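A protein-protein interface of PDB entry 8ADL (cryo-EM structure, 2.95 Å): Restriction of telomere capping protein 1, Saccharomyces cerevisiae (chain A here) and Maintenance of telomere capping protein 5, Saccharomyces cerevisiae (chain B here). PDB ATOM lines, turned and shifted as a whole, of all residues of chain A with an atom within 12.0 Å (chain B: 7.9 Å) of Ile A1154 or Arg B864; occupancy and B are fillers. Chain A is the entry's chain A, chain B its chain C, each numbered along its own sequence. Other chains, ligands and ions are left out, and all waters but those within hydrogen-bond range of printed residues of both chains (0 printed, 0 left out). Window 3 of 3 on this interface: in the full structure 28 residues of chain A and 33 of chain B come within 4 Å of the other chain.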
ATOM      1  N   ILE A1154     -14.942 -21.913  24.460  1.00  0.00           N
ATOM      2  CA  ILE A1154     -16.033 -21.495  25.328  1.00  0.00           C
ATOM      3  C   ILE A1154     -17.183 -20.971  24.461  1.00  0.00           C
ATOM      4  O   ILE A1154     -16.961 -20.397  23.392  1.00  0.00           O
ATOM      5  CB  ILE A1154     -15.542 -20.452  26.377  1.00  0.00           C
ATOM      6  CG1 ILE A1154     -16.607 -20.183  27.445  1.00  0.00           C
ATOM      7  CG2 ILE A1154     -15.080 -19.159  25.710  1.00  0.00           C
ATOM      8  CD1 ILE A1154     -16.089 -19.429  28.650  1.00  0.00           C
ATOM      9  N   ALA A1155     -18.416 -21.206  24.907  1.00  0.00           N
ATOM     10  CA  ALA A1155     -19.603 -20.770  24.190  1.00  0.00           C
ATOM     11  C   ALA A1155     -20.578 -20.147  25.177  1.00  0.00           C
ATOM     12  O   ALA A1155     -20.477 -20.344  26.390  1.00  0.00           O
ATOM     13  CB  ALA A1155     -20.271 -21.927  23.435  1.00  0.00           C
ATOM     14  N   ASP A1156     -21.524 -19.385  24.638  1.00  0.00           N
ATOM     15  CA  ASP A1156     -22.511 -18.720  25.470  1.00  0.00           C
ATOM     16  C   ASP A1156     -23.510 -19.733  26.031  1.00  0.00           C
ATOM     17  O   ASP A1156     -23.755 -20.778  25.422  1.00  0.00           O
ATOM     18  CB  ASP A1156     -23.245 -17.655  24.661  1.00  0.00           C
ATOM     19  CG  ASP A1156     -22.598 -16.290  24.776  1.00  0.00           C
ATOM     20  OD1 ASP A1156     -21.748 -16.110  25.672  1.00  0.00           O
ATOM     21  OD2 ASP A1156     -22.938 -15.399  23.970  1.00  0.00           O
ATOM     22  N   PRO A1157     -24.084 -19.458  27.200  1.00  0.00           N
ATOM     23  CA  PRO A1157     -25.107 -20.349  27.758  1.00  0.00           C
ATOM     24  C   PRO A1157     -26.382 -20.287  26.936  1.00  0.00           C
ATOM     25  O   PRO A1157     -26.624 -19.296  26.230  1.00  0.00           O
ATOM     26  CB  PRO A1157     -25.330 -19.793  29.174  1.00  0.00           C
ATOM     27  CG  PRO A1157     -24.113 -18.994  29.471  1.00  0.00           C
ATOM     28  CD  PRO A1157     -23.693 -18.413  28.163  1.00  0.00           C
ATOM     29  N   PRO A1158     -27.219 -21.329  26.986  1.00  0.00           N
ATOM     30  CA  PRO A1158     -28.480 -21.289  26.228  1.00  0.00           C
ATOM     31  C   PRO A1158     -29.493 -20.288  26.756  1.00  0.00           C
ATOM     32  O   PRO A1158     -30.429 -19.946  26.024  1.00  0.00           O
ATOM     33  CB  PRO A1158     -29.005 -22.724  26.347  1.00  0.00           C
ATOM     34  CG  PRO A1158     -28.377 -23.251  27.586  1.00  0.00           C
ATOM     35  CD  PRO A1158     -27.011 -22.637  27.632  1.00  0.00           C
ATOM     36  N   TRP A1159     -29.347 -19.806  27.988  1.00  0.00           N
ATOM     37  CA  TRP A1159     -30.254 -18.804  28.526  1.00  0.00           C
ATOM     38  C   TRP A1159     -29.739 -17.387  28.325  1.00  0.00           C
ATOM     39  O   TRP A1159     -30.304 -16.449  28.899  1.00  0.00           O
ATOM     40  CB  TRP A1159     -30.522 -19.059  30.009  1.00  0.00           C
ATOM     41  CG  TRP A1159     -29.292 -19.197  30.835  1.00  0.00           C
ATOM     42  CD1 TRP A1159     -28.583 -18.194  31.428  1.00  0.00           C
ATOM     43  CD2 TRP A1159     -28.623 -20.414  31.172  1.00  0.00           C
ATOM     44  NE1 TRP A1159     -27.512 -18.713  32.110  1.00  0.00           N
ATOM     45  CE2 TRP A1159     -27.514 -20.075  31.968  1.00  0.00           C
ATOM     46  CE3 TRP A1159     -28.853 -21.760  30.874  1.00  0.00           C
ATOM     47  CZ2 TRP A1159     -26.639 -21.031  32.470  1.00  0.00           C
ATOM     48  CZ3 TRP A1159     -27.985 -22.705  31.372  1.00  0.00           C
ATOM     49  CH2 TRP A1159     -26.892 -22.338  32.162  1.00  0.00           C
ATOM     50  N   ASP A1160     -28.665 -17.219  27.557  1.00  0.00           N
ATOM     51  CA  ASP A1160     -28.232 -15.892  27.144  1.00  0.00           C
ATOM     52  C   ASP A1160     -29.312 -15.255  26.279  1.00  0.00           C
ATOM     53  O   ASP A1160     -30.011 -15.937  25.526  1.00  0.00           O
ATOM     54  CB  ASP A1160     -26.914 -15.976  26.375  1.00  0.00           C
ATOM     55  CG  ASP A1160     -26.311 -14.616  26.101  1.00  0.00           C
ATOM     56  OD1 ASP A1160     -26.650 -13.656  26.824  1.00  0.00           O
ATOM     57  OD2 ASP A1160     -25.497 -14.505  25.161  1.00  0.00           O
ATOM     58  N   LYS A1163     -28.816 -15.393  22.307  1.00  0.00           N
ATOM     59  CA  LYS A1163     -28.884 -16.768  21.814  1.00  0.00           C
ATOM     60  C   LYS A1163     -30.290 -17.342  21.939  1.00  0.00           C
ATOM     61  O   LYS A1163     -30.786 -17.987  21.008  1.00  0.00           O
ATOM     62  CB  LYS A1163     -27.877 -17.645  22.556  1.00  0.00           C
ATOM     63  CG  LYS A1163     -27.600 -18.965  21.861  1.00  0.00           C
ATOM     64  CD  LYS A1163     -26.445 -19.703  22.510  1.00  0.00           C
ATOM     65  CE  LYS A1163     -26.205 -21.042  21.839  1.00  0.00           C
ATOM     66  NZ  LYS A1163     -25.101 -21.797  22.490  1.00  0.00           N
ATOM     67  N   GLU B 857     -27.695 -27.885  25.376  1.00  0.00           N
ATOM     68  CA  GLU B 857     -26.707 -26.826  25.556  1.00  0.00           C
ATOM     69  C   GLU B 857     -26.387 -26.598  27.027  1.00  0.00           C
ATOM     70  O   GLU B 857     -25.244 -26.272  27.365  1.00  0.00           O
ATOM     71  CB  GLU B 857     -27.192 -25.533  24.905  1.00  0.00           C
ATOM     72  CG  GLU B 857     -27.305 -25.598  23.393  1.00  0.00           C
ATOM     73  CD  GLU B 857     -25.971 -25.428  22.700  1.00  0.00           C
ATOM     74  OE1 GLU B 857     -25.056 -24.837  23.309  1.00  0.00           O
ATOM     75  OE2 GLU B 857     -25.837 -25.886  21.546  1.00  0.00           O
ATOM     76  N   ALA B 858     -27.367 -26.784  27.915  1.00  0.00           N
ATOM     77  CA  ALA B 858     -27.108 -26.653  29.344  1.00  0.00           C
ATOM     78  C   ALA B 858     -26.235 -27.791  29.857  1.00  0.00           C
ATOM     79  O   ALA B 858     -25.374 -27.572  30.716  1.00  0.00           O
ATOM     80  CB  ALA B 858     -28.428 -26.593  30.110  1.00  0.00           C
ATOM     81  N   ILE B 859     -26.447 -29.011  29.350  1.00  0.00           N
ATOM     82  CA  ILE B 859     -25.562 -30.128  29.677  1.00  0.00           C
ATOM     83  C   ILE B 859     -24.140 -29.852  29.210  1.00  0.00           C
ATOM     84  O   ILE B 859     -23.181 -30.103  29.948  1.00  0.00           O
ATOM     85  CB  ILE B 859     -26.119 -31.447  29.098  1.00  0.00           C
ATOM     86  CG1 ILE B 859     -27.382 -31.878  29.850  1.00  0.00           C
ATOM     87  CG2 ILE B 859     -25.072 -32.556  29.069  1.00  0.00           C
ATOM     88  CD1 ILE B 859     -28.125 -33.016  29.190  1.00  0.00           C
ATOM     89  N   VAL B 860     -23.977 -29.288  28.008  1.00  0.00           N
ATOM     90  CA  VAL B 860     -22.636 -28.941  27.524  1.00  0.00           C
ATOM     91  C   VAL B 860     -21.993 -27.871  28.410  1.00  0.00           C
ATOM     92  O   VAL B 860     -20.829 -27.995  28.829  1.00  0.00           O
ATOM     93  CB  VAL B 860     -22.698 -28.498  26.052  1.00  0.00           C
ATOM     94  CG1 VAL B 860     -21.372 -27.899  25.613  1.00  0.00           C
ATOM     95  CG2 VAL B 860     -23.063 -29.673  25.164  1.00  0.00           C
ATOM     96  N   TYR B 861     -22.762 -26.828  28.748  1.00  0.00           N
ATOM     97  CA  TYR B 861     -22.235 -25.714  29.533  1.00  0.00           C
ATOM     98  C   TYR B 861     -21.862 -26.140  30.948  1.00  0.00           C
ATOM     99  O   TYR B 861     -20.834 -25.705  31.480  1.00  0.00           O
ATOM    100  CB  TYR B 861     -23.257 -24.580  29.574  1.00  0.00           C
ATOM    101  CG  TYR B 861     -22.875 -23.437  30.484  1.00  0.00           C
ATOM    102  CD1 TYR B 861     -21.808 -22.602  30.180  1.00  0.00           C
ATOM    103  CD2 TYR B 861     -23.580 -23.198  31.655  1.00  0.00           C
ATOM    104  CE1 TYR B 861     -21.460 -21.556  31.018  1.00  0.00           C
ATOM    105  CE2 TYR B 861     -23.240 -22.157  32.496  1.00  0.00           C
ATOM    106  CZ  TYR B 861     -22.181 -21.341  32.173  1.00  0.00           C
ATOM    107  OH  TYR B 861     -21.845 -20.306  33.014  1.00  0.00           O
ATOM    108  N   PHE B 862     -22.677 -26.987  31.575  1.00  0.00           N
ATOM    109  CA  PHE B 862     -22.377 -27.435  32.927  1.00  0.00           C
ATOM    110  C   PHE B 862     -21.392 -28.595  32.951  1.00  0.00           C
ATOM    111  O   PHE B 862     -20.818 -28.879  34.008  1.00  0.00           O
ATOM    112  CB  PHE B 862     -23.674 -27.798  33.649  1.00  0.00           C
ATOM    113  CG  PHE B 862     -24.472 -26.599  34.076  1.00  0.00           C
ATOM    114  CD1 PHE B 862     -23.908 -25.640  34.900  1.00  0.00           C
ATOM    115  CD2 PHE B 862     -25.768 -26.412  33.629  1.00  0.00           C
ATOM    116  CE1 PHE B 862     -24.630 -24.530  35.292  1.00  0.00           C
ATOM    117  CE2 PHE B 862     -26.493 -25.301  34.010  1.00  0.00           C
ATOM    118  CZ  PHE B 862     -25.923 -24.362  34.847  1.00  0.00           C
ATOM    119  N   GLU B 863     -21.185 -29.272  31.819  1.00  0.00           N
ATOM    120  CA  GLU B 863     -20.032 -30.152  31.689  1.00  0.00           C
ATOM    121  C   GLU B 863     -18.743 -29.346  31.684  1.00  0.00           C
ATOM    122  O   GLU B 863     -17.757 -29.741  32.318  1.00  0.00           O
ATOM    123  CB  GLU B 863     -20.146 -30.991  30.418  1.00  0.00           C
ATOM    124  CG  GLU B 863     -20.881 -32.306  30.597  1.00  0.00           C
ATOM    125  CD  GLU B 863     -21.263 -32.937  29.272  1.00  0.00           C
ATOM    126  OE1 GLU B 863     -21.095 -32.273  28.228  1.00  0.00           O
ATOM    127  OE2 GLU B 863     -21.732 -34.094  29.273  1.00  0.00           O
ATOM    128  N   ARG B 864     -18.725 -28.217  30.967  1.00  0.00           N
ATOM    129  CA  ARG B 864     -17.529 -27.382  30.985  1.00  0.00           C
ATOM    130  C   ARG B 864     -17.333 -26.676  32.323  1.00  0.00           C
ATOM    131  O   ARG B 864     -16.204 -26.291  32.643  1.00  0.00           O
ATOM    132  CB  ARG B 864     -17.563 -26.359  29.850  1.00  0.00           C
ATOM    133  CG  ARG B 864     -17.359 -26.973  28.475  1.00  0.00           C
ATOM    134  CD  ARG B 864     -17.504 -25.938  27.375  1.00  0.00           C
ATOM    135  NE  ARG B 864     -18.666 -25.081  27.569  1.00  0.00           N
ATOM    136  CZ  ARG B 864     -19.171 -24.288  26.635  1.00  0.00           C
ATOM    137  NH1 ARG B 864     -18.645 -24.228  25.423  1.00  0.00           N
ATOM    138  NH2 ARG B 864     -20.231 -23.538  26.924  1.00  0.00           N
ATOM    139  N   GLN B 865     -18.394 -26.501  33.107  1.00  0.00           N
ATOM    140  CA  GLN B 865     -18.293 -25.864  34.414  1.00  0.00           C
ATOM    141  C   GLN B 865     -18.038 -26.865  35.533  1.00  0.00           C
ATOM    142  O   GLN B 865     -17.861 -26.445  36.683  1.00  0.00           O
ATOM    143  CB  GLN B 865     -19.572 -25.079  34.724  1.00  0.00           C
ATOM    144  CG  GLN B 865     -19.715 -23.772  33.970  1.00  0.00           C
ATOM    145  CD  GLN B 865     -18.734 -22.719  34.442  1.00  0.00           C
ATOM    146  OE1 GLN B 865     -17.814 -22.344  33.717  1.00  0.00           O
ATOM    147  NE2 GLN B 865     -18.927 -22.235  35.663  1.00  0.00           N
ATOM    148  N   GLN B 866     -18.019 -28.166  35.210  1.00  0.00           N
ATOM    149  CA  GLN B 866     -17.816 -29.265  36.165  1.00  0.00           C
ATOM    150  C   GLN B 866     -18.844 -29.224  37.298  1.00  0.00           C
ATOM    151  O   GLN B 866     -18.501 -29.212  38.482  1.00  0.00           O
ATOM    152  CB  GLN B 866     -16.386 -29.267  36.713  1.00  0.00           C
ATOM    153  CG  GLN B 866     -15.314 -29.313  35.632  1.00  0.00           C
ATOM    154  CD  GLN B 866     -15.013 -30.722  35.165  1.00  0.00           C
ATOM    155  OE1 GLN B 866     -15.308 -31.695  35.858  1.00  0.00           O
ATOM    156  NE2 GLN B 866     -14.424 -30.839  33.980  1.00  0.00           N
ATOM    157  N   ASN B 867     -20.121 -29.204  36.923  1.00  0.00           N
ATOM    158  CA  ASN B 867     -21.233 -29.157  37.871  1.00  0.00           C
ATOM    159  C   ASN B 867     -22.074 -30.418  37.684  1.00  0.00           C
ATOM    160  O   ASN B 867     -23.034 -30.432  36.908  1.00  0.00           O
ATOM    161  CB  ASN B 867     -22.060 -27.890  37.683  1.00  0.00           C
ATOM    162  CG  ASN B 867     -22.793 -27.482  38.945  1.00  0.00           C
ATOM    163  OD1 ASN B 867     -23.307 -28.325  39.679  1.00  0.00           O
ATOM    164  ND2 ASN B 867     -22.839 -26.182  39.207  1.00  0.00           N
ATOM    165  N   LEU B 871     -26.086 -31.026  36.485  1.00  0.00           N
ATOM    166  CA  LEU B 871     -26.278 -31.957  35.374  1.00  0.00           C
ATOM    167  C   LEU B 871     -27.342 -32.998  35.705  1.00  0.00           C
ATOM    168  O   LEU B 871     -28.318 -33.174  34.959  1.00  0.00           O
ATOM    169  CB  LEU B 871     -24.953 -32.647  35.054  1.00  0.00           C
ATOM    170  CG  LEU B 871     -24.008 -31.977  34.065  1.00  0.00           C
ATOM    171  CD1 LEU B 871     -22.630 -32.607  34.147  1.00  0.00           C
ATOM    172  CD2 LEU B 871     -24.563 -32.108  32.678  1.00  0.00           C
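The backbone carbonyl oxygen (O) of Asp A1156 is in hydrogen-bond range of the side-chain amino group (NZ) of Lys A1163. The backbone NH (N) of Asn B867 lies within hydrogen-bond range of the backbone carbonyl oxygen (O) of Phe B862 (3.0 Å).
Ile A1154 touches Arg B864. Tyr B861 touches Pro A1157 (CE1 to CG, 3.999 Å). Glu B857 touches Pro A1158 (CB to CB, 3.6 Å). CG of Pro A1158 touches N of Ala B858 (3.7 Å). Tyr B861 touches Trp A1159 (CD2 to CH2, 3.5 Å). Phe B862 touches Trp A1159.
Of chain B, only Arg B864 comes within 4 Å of Ile A1154. Of the printed residues of chain B, Pro A1158 touches Glu B857 and Ala B858. No residue of chain A comes within 4 Å of Val B860. Of the printed residues of chain A, Tyr B861 touches Pro A1157 and Trp A1159. No residue of chain A comes within 4 Å of Glu B863. Arg B864 touches just these residues of chain A: Ile A1154 (3.7 Å) and Ala A1155 (3.1 Å). Gln B865 touches none of the printed residues of chain A. No residue of chain A comes within 4 Å of Gln B866. The nearest residue of chain B that does not touch Ile A1154 is Gln B865 (6.1 Å). The nearest residue of chain A that does not touch Arg B864 is Asp A1156 (4.7 Å). The nearest printed residue of chain B that does not touch Pro A1158 is Tyr B861 (4.7 Å).
Printed residues of chain A that touch a printed residue of chain B: Ile A1154, Ala A1155, Pro A1157, Pro A1158, Trp A1159 and Lys A1163.
The guanidinium group of Arg B864 sits at hydrogen-bond distance from the backbone carbonyl oxygen of Ala A1155. NZ of Lys A1163 lies within salt-bridge range of OE1 of Glu B857 (3.1 Å).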
